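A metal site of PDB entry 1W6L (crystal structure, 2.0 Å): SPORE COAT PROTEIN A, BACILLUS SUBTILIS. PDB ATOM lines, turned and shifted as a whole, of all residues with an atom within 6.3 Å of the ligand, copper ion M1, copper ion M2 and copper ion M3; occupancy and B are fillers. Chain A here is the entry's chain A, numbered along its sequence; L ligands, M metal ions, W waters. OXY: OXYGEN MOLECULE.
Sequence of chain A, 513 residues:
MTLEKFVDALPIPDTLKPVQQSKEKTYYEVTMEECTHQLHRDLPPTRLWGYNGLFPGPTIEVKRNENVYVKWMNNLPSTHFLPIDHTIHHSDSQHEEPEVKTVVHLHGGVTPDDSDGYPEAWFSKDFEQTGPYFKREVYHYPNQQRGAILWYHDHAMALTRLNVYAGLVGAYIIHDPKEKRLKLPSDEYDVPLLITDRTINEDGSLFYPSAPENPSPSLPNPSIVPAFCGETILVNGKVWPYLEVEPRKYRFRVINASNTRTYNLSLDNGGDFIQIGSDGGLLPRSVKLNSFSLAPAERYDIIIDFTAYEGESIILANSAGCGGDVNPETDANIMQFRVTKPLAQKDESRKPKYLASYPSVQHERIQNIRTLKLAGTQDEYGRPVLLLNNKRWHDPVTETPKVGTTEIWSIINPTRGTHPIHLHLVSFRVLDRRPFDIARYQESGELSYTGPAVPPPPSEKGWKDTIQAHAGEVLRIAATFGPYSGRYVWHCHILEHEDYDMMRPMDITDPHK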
ATOM      1  N   HIS A 105      -0.711   3.254  26.572  1.00  0.00           N
ATOM      2  CA  HIS A 105      -2.134   3.492  26.800  1.00  0.00           C
ATOM      3  C   HIS A 105      -2.904   2.175  26.751  1.00  0.00           C
ATOM      4  O   HIS A 105      -2.769   1.399  25.765  1.00  0.00           O
ATOM      5  CB  HIS A 105      -2.673   4.452  25.744  1.00  0.00           C
ATOM      6  CG  HIS A 105      -4.170   4.601  25.749  1.00  0.00           C
ATOM      7  ND1 HIS A 105      -4.883   4.919  26.896  1.00  0.00           N
ATOM      8  CD2 HIS A 105      -5.094   4.449  24.768  1.00  0.00           C
ATOM      9  CE1 HIS A 105      -6.170   5.005  26.594  1.00  0.00           C
ATOM     10  NE2 HIS A 105      -6.325   4.712  25.313  1.00  0.00           N
ATOM     11  N   LEU A 106      -3.703   1.910  27.782  1.00  0.00           N
ATOM     12  CA  LEU A 106      -4.630   0.794  27.762  1.00  0.00           C
ATOM     13  C   LEU A 106      -5.952   1.296  27.187  1.00  0.00           C
ATOM     14  O   LEU A 106      -6.731   1.973  27.849  1.00  0.00           O
ATOM     15  CB  LEU A 106      -4.843   0.211  29.130  1.00  0.00           C
ATOM     16  CG  LEU A 106      -5.867  -0.918  29.210  1.00  0.00           C
ATOM     17  CD1 LEU A 106      -5.472  -2.160  28.358  1.00  0.00           C
ATOM     18  CD2 LEU A 106      -6.049  -1.311  30.613  1.00  0.00           C
ATOM     19  N   HIS A 107      -6.137   1.025  25.887  1.00  0.00           N
ATOM     20  CA  HIS A 107      -7.299   1.448  25.158  1.00  0.00           C
ATOM     21  C   HIS A 107      -8.572   0.736  25.654  1.00  0.00           C
ATOM     22  O   HIS A 107      -8.642  -0.502  25.655  1.00  0.00           O
ATOM     23  CB  HIS A 107      -7.069   1.217  23.683  1.00  0.00           C
ATOM     24  CG  HIS A 107      -8.155   1.742  22.827  1.00  0.00           C
ATOM     25  ND1 HIS A 107      -7.925   2.513  21.728  1.00  0.00           N
ATOM     26  CD2 HIS A 107      -9.509   1.578  22.903  1.00  0.00           C
ATOM     27  CE1 HIS A 107      -9.083   2.840  21.166  1.00  0.00           C
ATOM     28  NE2 HIS A 107     -10.057   2.269  21.859  1.00  0.00           N
ATOM     29  N   GLY A 108      -9.532   1.556  26.103  1.00  0.00           N
ATOM     30  CA  GLY A 108     -10.776   1.091  26.737  1.00  0.00           C
ATOM     31  C   GLY A 108     -10.702   1.056  28.251  1.00  0.00           C
ATOM     32  O   GLY A 108     -11.679   0.724  28.950  1.00  0.00           O
ATOM     33  N   GLY A 109      -9.509   1.315  28.803  1.00  0.00           N
ATOM     34  CA  GLY A 109      -9.326   1.180  30.211  1.00  0.00           C
ATOM     35  C   GLY A 109     -10.064   2.270  30.960  1.00  0.00           C
ATOM     36  O   GLY A 109      -9.993   3.432  30.569  1.00  0.00           O
ATOM     37  N   ASP A 116      -3.228   6.577  32.389  1.00  0.00           N
ATOM     38  CA  ASP A 116      -3.930   6.437  31.102  1.00  0.00           C
ATOM     39  C   ASP A 116      -2.990   6.523  29.872  1.00  0.00           C
ATOM     40  O   ASP A 116      -3.350   6.111  28.747  1.00  0.00           O
ATOM     41  CB  ASP A 116      -5.065   7.475  31.030  1.00  0.00           C
ATOM     42  CG  ASP A 116      -6.019   7.212  29.878  1.00  0.00           C
ATOM     43  OD1 ASP A 116      -6.528   6.057  29.798  1.00  0.00           O
ATOM     44  OD2 ASP A 116      -6.318   8.085  29.048  1.00  0.00           O
ATOM     45  N   TRP A 151      -7.050  -3.324  24.486  1.00  0.00           N
ATOM     46  CA  TRP A 151      -5.752  -3.526  23.885  1.00  0.00           C
ATOM     47  C   TRP A 151      -4.838  -2.399  24.314  1.00  0.00           C
ATOM     48  O   TRP A 151      -5.323  -1.318  24.682  1.00  0.00           O
ATOM     49  CB  TRP A 151      -5.837  -3.697  22.362  1.00  0.00           C
ATOM     50  CG  TRP A 151      -6.232  -2.503  21.534  1.00  0.00           C
ATOM     51  CD1 TRP A 151      -7.445  -1.844  21.551  1.00  0.00           C
ATOM     52  CD2 TRP A 151      -5.447  -1.863  20.515  1.00  0.00           C
ATOM     53  NE1 TRP A 151      -7.444  -0.835  20.619  1.00  0.00           N
ATOM     54  CE2 TRP A 151      -6.234  -0.820  19.963  1.00  0.00           C
ATOM     55  CE3 TRP A 151      -4.139  -2.049  20.009  1.00  0.00           C
ATOM     56  CZ2 TRP A 151      -5.753   0.040  18.978  1.00  0.00           C
ATOM     57  CZ3 TRP A 151      -3.675  -1.214  19.021  1.00  0.00           C
ATOM     58  CH2 TRP A 151      -4.474  -0.170  18.517  1.00  0.00           C
ATOM     59  N   HIS A 153      -1.183  -0.088  23.668  1.00  0.00           N
ATOM     60  CA  HIS A 153      -0.333   0.388  22.595  1.00  0.00           C
ATOM     61  C   HIS A 153       0.352   1.687  22.974  1.00  0.00           C
ATOM     62  O   HIS A 153      -0.042   2.356  23.927  1.00  0.00           O
ATOM     63  CB  HIS A 153      -1.105   0.521  21.276  1.00  0.00           C
ATOM     64  CG  HIS A 153      -2.187   1.561  21.290  1.00  0.00           C
ATOM     65  ND1 HIS A 153      -1.921   2.898  21.069  1.00  0.00           N
ATOM     66  CD2 HIS A 153      -3.534   1.454  21.439  1.00  0.00           C
ATOM     67  CE1 HIS A 153      -3.062   3.572  21.083  1.00  0.00           C
ATOM     68  NE2 HIS A 153      -4.053   2.720  21.322  1.00  0.00           N
ATOM     69  N   ASP A 154       1.381   2.041  22.226  1.00  0.00           N
ATOM     70  CA  ASP A 154       2.105   3.261  22.492  1.00  0.00           C
ATOM     71  C   ASP A 154       1.260   4.488  22.160  1.00  0.00           C
ATOM     72  O   ASP A 154       0.443   4.450  21.245  1.00  0.00           O
ATOM     73  CB  ASP A 154       3.419   3.312  21.717  1.00  0.00           C
ATOM     74  CG  ASP A 154       4.305   4.436  22.200  1.00  0.00           C
ATOM     75  OD1 ASP A 154       4.293   5.519  21.552  1.00  0.00           O
ATOM     76  OD2 ASP A 154       4.978   4.307  23.246  1.00  0.00           O
ATOM     77  N   HIS A 155       1.458   5.578  22.894  1.00  0.00           N
ATOM     78  CA  HIS A 155       0.645   6.795  22.746  1.00  0.00           C
ATOM     79  C   HIS A 155       1.517   8.074  22.780  1.00  0.00           C
ATOM     80  O   HIS A 155       0.993   9.165  22.994  1.00  0.00           O
ATOM     81  CB  HIS A 155      -0.462   6.881  23.828  1.00  0.00           C
ATOM     82  CG  HIS A 155      -1.722   7.519  23.360  1.00  0.00           C
ATOM     83  ND1 HIS A 155      -1.748   8.672  22.615  1.00  0.00           N
ATOM     84  CD2 HIS A 155      -3.023   7.137  23.484  1.00  0.00           C
ATOM     85  CE1 HIS A 155      -2.998   8.983  22.319  1.00  0.00           C
ATOM     86  NE2 HIS A 155      -3.794   8.076  22.844  1.00  0.00           N
ATOM     87  N   THR A 160       3.224   8.407  17.759  1.00  0.00           N
ATOM     88  CA  THR A 160       2.317   7.264  17.920  1.00  0.00           C
ATOM     89  C   THR A 160       2.226   6.357  16.673  1.00  0.00           C
ATOM     90  O   THR A 160       2.261   5.120  16.793  1.00  0.00           O
ATOM     91  CB  THR A 160       0.927   7.797  18.348  1.00  0.00           C
ATOM     92  OG1 THR A 160       1.042   8.331  19.689  1.00  0.00           O
ATOM     93  CG2 THR A 160      -0.082   6.719  18.504  1.00  0.00           C
ATOM     94  N   ALA A 297      -8.782   0.559  15.811  1.00  0.00           N
ATOM     95  CA  ALA A 297      -9.105   0.478  17.227  1.00  0.00           C
ATOM     96  C   ALA A 297     -10.467  -0.066  17.595  1.00  0.00           C
ATOM     97  O   ALA A 297     -10.706  -0.298  18.776  1.00  0.00           O
ATOM     98  CB  ALA A 297      -8.855   1.846  17.949  1.00  0.00           C
ATOM     99  N   HIS A 422     -12.365   8.391  18.781  1.00  0.00           N
ATOM    100  CA  HIS A 422     -12.204   7.712  20.026  1.00  0.00           C
ATOM    101  C   HIS A 422     -12.148   8.708  21.211  1.00  0.00           C
ATOM    102  O   HIS A 422     -11.429   9.726  21.170  1.00  0.00           O
ATOM    103  CB  HIS A 422     -10.940   6.878  19.932  1.00  0.00           C
ATOM    104  CG  HIS A 422     -10.513   6.242  21.203  1.00  0.00           C
ATOM    105  ND1 HIS A 422     -11.350   5.489  21.994  1.00  0.00           N
ATOM    106  CD2 HIS A 422      -9.304   6.233  21.814  1.00  0.00           C
ATOM    107  CE1 HIS A 422     -10.691   5.092  23.072  1.00  0.00           C
ATOM    108  NE2 HIS A 422      -9.448   5.551  22.994  1.00  0.00           N
ATOM    109  N   LEU A 423     -12.884   8.378  22.259  1.00  0.00           N
ATOM    110  CA  LEU A 423     -12.783   9.058  23.553  1.00  0.00           C
ATOM    111  C   LEU A 423     -12.117   8.144  24.567  1.00  0.00           C
ATOM    112  O   LEU A 423     -12.508   7.000  24.724  1.00  0.00           O
ATOM    113  CB  LEU A 423     -14.187   9.434  24.062  1.00  0.00           C
ATOM    114  CG  LEU A 423     -14.865  10.695  23.503  1.00  0.00           C
ATOM    115  CD1 LEU A 423     -15.021  10.617  21.971  1.00  0.00           C
ATOM    116  CD2 LEU A 423     -16.232  10.881  24.190  1.00  0.00           C
ATOM    117  N   HIS A 424     -11.151   8.658  25.317  1.00  0.00           N
ATOM    118  CA  HIS A 424     -10.587   7.933  26.448  1.00  0.00           C
ATOM    119  C   HIS A 424     -11.558   7.864  27.608  1.00  0.00           C
ATOM    120  O   HIS A 424     -12.566   8.573  27.624  1.00  0.00           O
ATOM    121  CB  HIS A 424      -9.274   8.567  26.921  1.00  0.00           C
ATOM    122  CG  HIS A 424      -8.123   8.334  26.006  1.00  0.00           C
ATOM    123  ND1 HIS A 424      -6.826   8.188  26.446  1.00  0.00           N
ATOM    124  CD2 HIS A 424      -8.079   8.238  24.647  1.00  0.00           C
ATOM    125  CE1 HIS A 424      -6.040   8.000  25.397  1.00  0.00           C
ATOM    126  NE2 HIS A 424      -6.775   8.032  24.296  1.00  0.00           N
ATOM    127  N   LEU A 425     -11.243   6.957  28.525  1.00  0.00           N
ATOM    128  CA  LEU A 425     -11.935   6.664  29.789  1.00  0.00           C
ATOM    129  C   LEU A 425     -13.316   5.989  29.660  1.00  0.00           C
ATOM    130  O   LEU A 425     -13.581   4.970  30.309  1.00  0.00           O
ATOM    131  CB  LEU A 425     -12.048   7.925  30.690  1.00  0.00           C
ATOM    132  CG  LEU A 425     -12.702   7.699  32.066  1.00  0.00           C
ATOM    133  CD1 LEU A 425     -11.870   6.823  32.916  1.00  0.00           C
ATOM    134  CD2 LEU A 425     -13.029   9.011  32.790  1.00  0.00           C
ATOM    135  N   ASP A 465     -16.384   2.659  22.148  1.00  0.00           N
ATOM    136  CA  ASP A 465     -15.392   3.707  22.453  1.00  0.00           C
ATOM    137  C   ASP A 465     -14.658   4.282  21.278  1.00  0.00           C
ATOM    138  O   ASP A 465     -13.994   5.312  21.387  1.00  0.00           O
ATOM    139  CB  ASP A 465     -14.442   3.279  23.563  1.00  0.00           C
ATOM    140  CG  ASP A 465     -13.458   2.190  23.144  1.00  0.00           C
ATOM    141  OD1 ASP A 465     -12.883   2.215  22.030  1.00  0.00           O
ATOM    142  OD2 ASP A 465     -13.180   1.305  23.979  1.00  0.00           O
ATOM    143  N   THR A 466     -14.818   3.656  20.113  1.00  0.00           N
ATOM    144  CA  THR A 466     -14.221   4.133  18.884  1.00  0.00           C
ATOM    145  C   THR A 466     -15.337   3.980  17.834  1.00  0.00           C
ATOM    146  O   THR A 466     -15.883   2.884  17.673  1.00  0.00           O
ATOM    147  CB  THR A 466     -13.012   3.291  18.508  1.00  0.00           C
ATOM    148  OG1 THR A 466     -12.018   3.331  19.550  1.00  0.00           O
ATOM    149  CG2 THR A 466     -12.306   3.864  17.295  1.00  0.00           C
ATOM    150  N   VAL A 489      -7.870  12.481  26.792  1.00  0.00           N
ATOM    151  CA  VAL A 489      -7.806  12.945  25.410  1.00  0.00           C
ATOM    152  C   VAL A 489      -8.972  12.357  24.632  1.00  0.00           C
ATOM    153  O   VAL A 489      -9.628  11.405  25.111  1.00  0.00           O
ATOM    154  CB  VAL A 489      -6.451  12.608  24.671  1.00  0.00           C
ATOM    155  CG1 VAL A 489      -5.249  13.146  25.468  1.00  0.00           C
ATOM    156  CG2 VAL A 489      -6.277  11.117  24.458  1.00  0.00           C
ATOM    157  N   HIS A 491      -9.690  11.812  20.152  1.00  0.00           N
ATOM    158  CA  HIS A 491      -9.005  11.907  18.888  1.00  0.00           C
ATOM    159  C   HIS A 491      -9.482  10.967  17.814  1.00  0.00           C
ATOM    160  O   HIS A 491     -10.166   9.979  18.080  1.00  0.00           O
ATOM    161  CB  HIS A 491      -7.529  11.641  19.045  1.00  0.00           C
ATOM    162  CG  HIS A 491      -7.189  10.303  19.623  1.00  0.00           C
ATOM    163  ND1 HIS A 491      -6.774   9.252  18.846  1.00  0.00           N
ATOM    164  CD2 HIS A 491      -7.208   9.849  20.904  1.00  0.00           C
ATOM    165  CE1 HIS A 491      -6.495   8.220  19.631  1.00  0.00           C
ATOM    166  NE2 HIS A 491      -6.724   8.566  20.878  1.00  0.00           N
ATOM    167  N   HIS A 493      -8.531   7.948  15.498  1.00  0.00           N
ATOM    168  CA  HIS A 493      -7.640   6.781  15.707  1.00  0.00           C
ATOM    169  C   HIS A 493      -6.960   6.302  14.420  1.00  0.00           C
ATOM    170  O   HIS A 493      -6.300   5.252  14.404  1.00  0.00           O
ATOM    171  CB  HIS A 493      -8.327   5.586  16.449  1.00  0.00           C
ATOM    172  CG  HIS A 493      -7.393   4.846  17.395  1.00  0.00           C
ATOM    173  ND1 HIS A 493      -6.185   4.341  16.982  1.00  0.00           N
ATOM    174  CD2 HIS A 493      -7.490   4.531  18.715  1.00  0.00           C
ATOM    175  CE1 HIS A 493      -5.569   3.765  18.010  1.00  0.00           C
ATOM    176  NE2 HIS A 493      -6.333   3.878  19.065  1.00  0.00           N
ATOM    177  N   LEU A 495      -3.801   6.903  12.943  1.00  0.00           N
ATOM    178  CA  LEU A 495      -2.627   7.387  13.662  1.00  0.00           C
ATOM    179  C   LEU A 495      -1.903   8.511  12.930  1.00  0.00           C
ATOM    180  O   LEU A 495      -1.403   9.440  13.557  1.00  0.00           O
ATOM    181  CB  LEU A 495      -1.671   6.234  13.990  1.00  0.00           C
ATOM    182  CG  LEU A 495      -2.311   5.082  14.806  1.00  0.00           C
ATOM    183  CD1 LEU A 495      -1.267   4.063  15.226  1.00  0.00           C
ATOM    184  CD2 LEU A 495      -3.039   5.604  16.008  1.00  0.00           C
ATOM    185  N   GLU A 498      -4.074  11.467  13.932  1.00  0.00           N
ATOM    186  CA  GLU A 498      -3.795  11.700  15.338  1.00  0.00           C
ATOM    187  C   GLU A 498      -2.509  12.501  15.586  1.00  0.00           C
ATOM    188  O   GLU A 498      -2.518  13.450  16.384  1.00  0.00           O
ATOM    189  CB  GLU A 498      -3.766  10.366  16.086  1.00  0.00           C
ATOM    190  CG  GLU A 498      -3.315  10.449  17.538  1.00  0.00           C
ATOM    191  CD  GLU A 498      -3.410   9.124  18.266  1.00  0.00           C
ATOM    192  OE1 GLU A 498      -4.115   8.219  17.783  1.00  0.00           O
ATOM    193  OE2 GLU A 498      -2.784   8.996  19.352  1.00  0.00           O
ATOM    194  N   MET A 503      -6.131  15.491  17.544  1.00  0.00           N
ATOM    195  CA  MET A 503      -6.195  15.005  18.917  1.00  0.00           C
ATOM    196  C   MET A 503      -6.292  16.233  19.813  1.00  0.00           C
ATOM    197  O   MET A 503      -5.626  17.254  19.562  1.00  0.00           O
ATOM    198  CB  MET A 503      -4.913  14.218  19.249  1.00  0.00           C
ATOM    199  CG  MET A 503      -4.883  13.677  20.686  1.00  0.00           C
ATOM    200  SD  MET A 503      -3.542  12.541  21.038  1.00  0.00           S
ATOM    201  CE  MET A 503      -2.096  13.520  20.839  1.00  0.00           C
HETATM  202  O1  OXY L   1      -5.509   5.652  21.441  1.00  0.00           O
HETATM  203  O2  OXY L   1      -6.269   5.421  22.316  1.00  0.00           O
HETATM  204 CU    CU M   1      -6.067   3.170  21.060  1.00  0.00          CU
HETATM  205 CU    CU M   2      -5.839   7.653  22.515  1.00  0.00          CU
HETATM  206 CU    CU M   3      -7.837   5.030  24.105  1.00  0.00          CU
HETATM  207  O   HOH W   1      -3.780   6.355  19.925  1.00  0.00           O
HETATM  208  O   HOH W   2      -9.603   4.357  26.416  1.00  0.00           O
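A ring nitrogen (ND1) of His 155 sits close to the side-chain carboxylate (OE2) of Glu 498, 3.4 Å away. N of His 105 sits at hydrogen-bond distance from O of His 153 (2.9 Å). O of Trp 151 sits at hydrogen-bond distance from N of His 107 (2.8 Å). A ring nitrogen (ND1) of His 422 lies within hydrogen-bond range of the backbone carbonyl oxygen (O) of Asp 465, 2.7 Å away. The backbone carbonyl oxygen (O) of His 155 lies close to the side-chain hydroxyl (OG1) of Thr 160 (3.4 Å). A ring nitrogen (ND1) of His 105 lies within hydrogen-bond range of the backbone carbonyl oxygen (O) of Asp 116, at 2.7 Å. A ring nitrogen (NE2) of His 107 is in hydrogen-bond range of the side-chain hydroxyl (OG1) of Thr 466 (3.2 Å). The side-chain carboxylate (OD2) of Asp 116 lies within hydrogen-bond range of a ring nitrogen (ND1) of His 424.
Hydrophobic or aromatic side chains that line the ligand: His 105, His 107, His 153, His 155, His 422, His 491 and His 493. Of the 24 residues printed, 8 come within 4 Å of the ligand. The nearest printed residue that does not touch the ligand is Glu 498 (4.7 Å).
Merely in contact with copper ion M1: Trp 151. Of the 24 residues printed, 4 come within 4 Å of copper ion M1.
Val 489 touches copper ion M2. Within 4 Å of copper ion M2: His 105, His 155, His 422, His 424, Val 489 and His 491. The nearest printed residue that does not touch copper ion M2 is Glu 498 (4.6 Å).
Four residues have an atom within 4 Å of copper ion M3: His 105, His 107, His 422 and His 424.
Copper ion M1 is bound by a ring nitrogen (NE2) of His 153 (2.1 Å), a ring nitrogen (ND1) of His 107 (2.1 Å), a ring nitrogen (NE2) of His 493 (2.1 Å) and an oxygen (O1) of the ligand (2.6 Å). Copper ion M1 has four donor atoms within binding distance.
Copper ion M2 is bound by NE2 of His 424 (2.0 Å), NE2 of His 491 (2.1 Å), NE2 of His 155 (2.1 Å) and O2 of the ligand (2.3 Å).
Copper ion M3 is bound by a ring nitrogen (NE2) of His 105 (2.0 Å), a ring nitrogen (NE2) of His 422 (2.0 Å) and an oxygen (O2) of the ligand (2.4 Å). Copper ion M3 has three donor atoms within binding distance.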
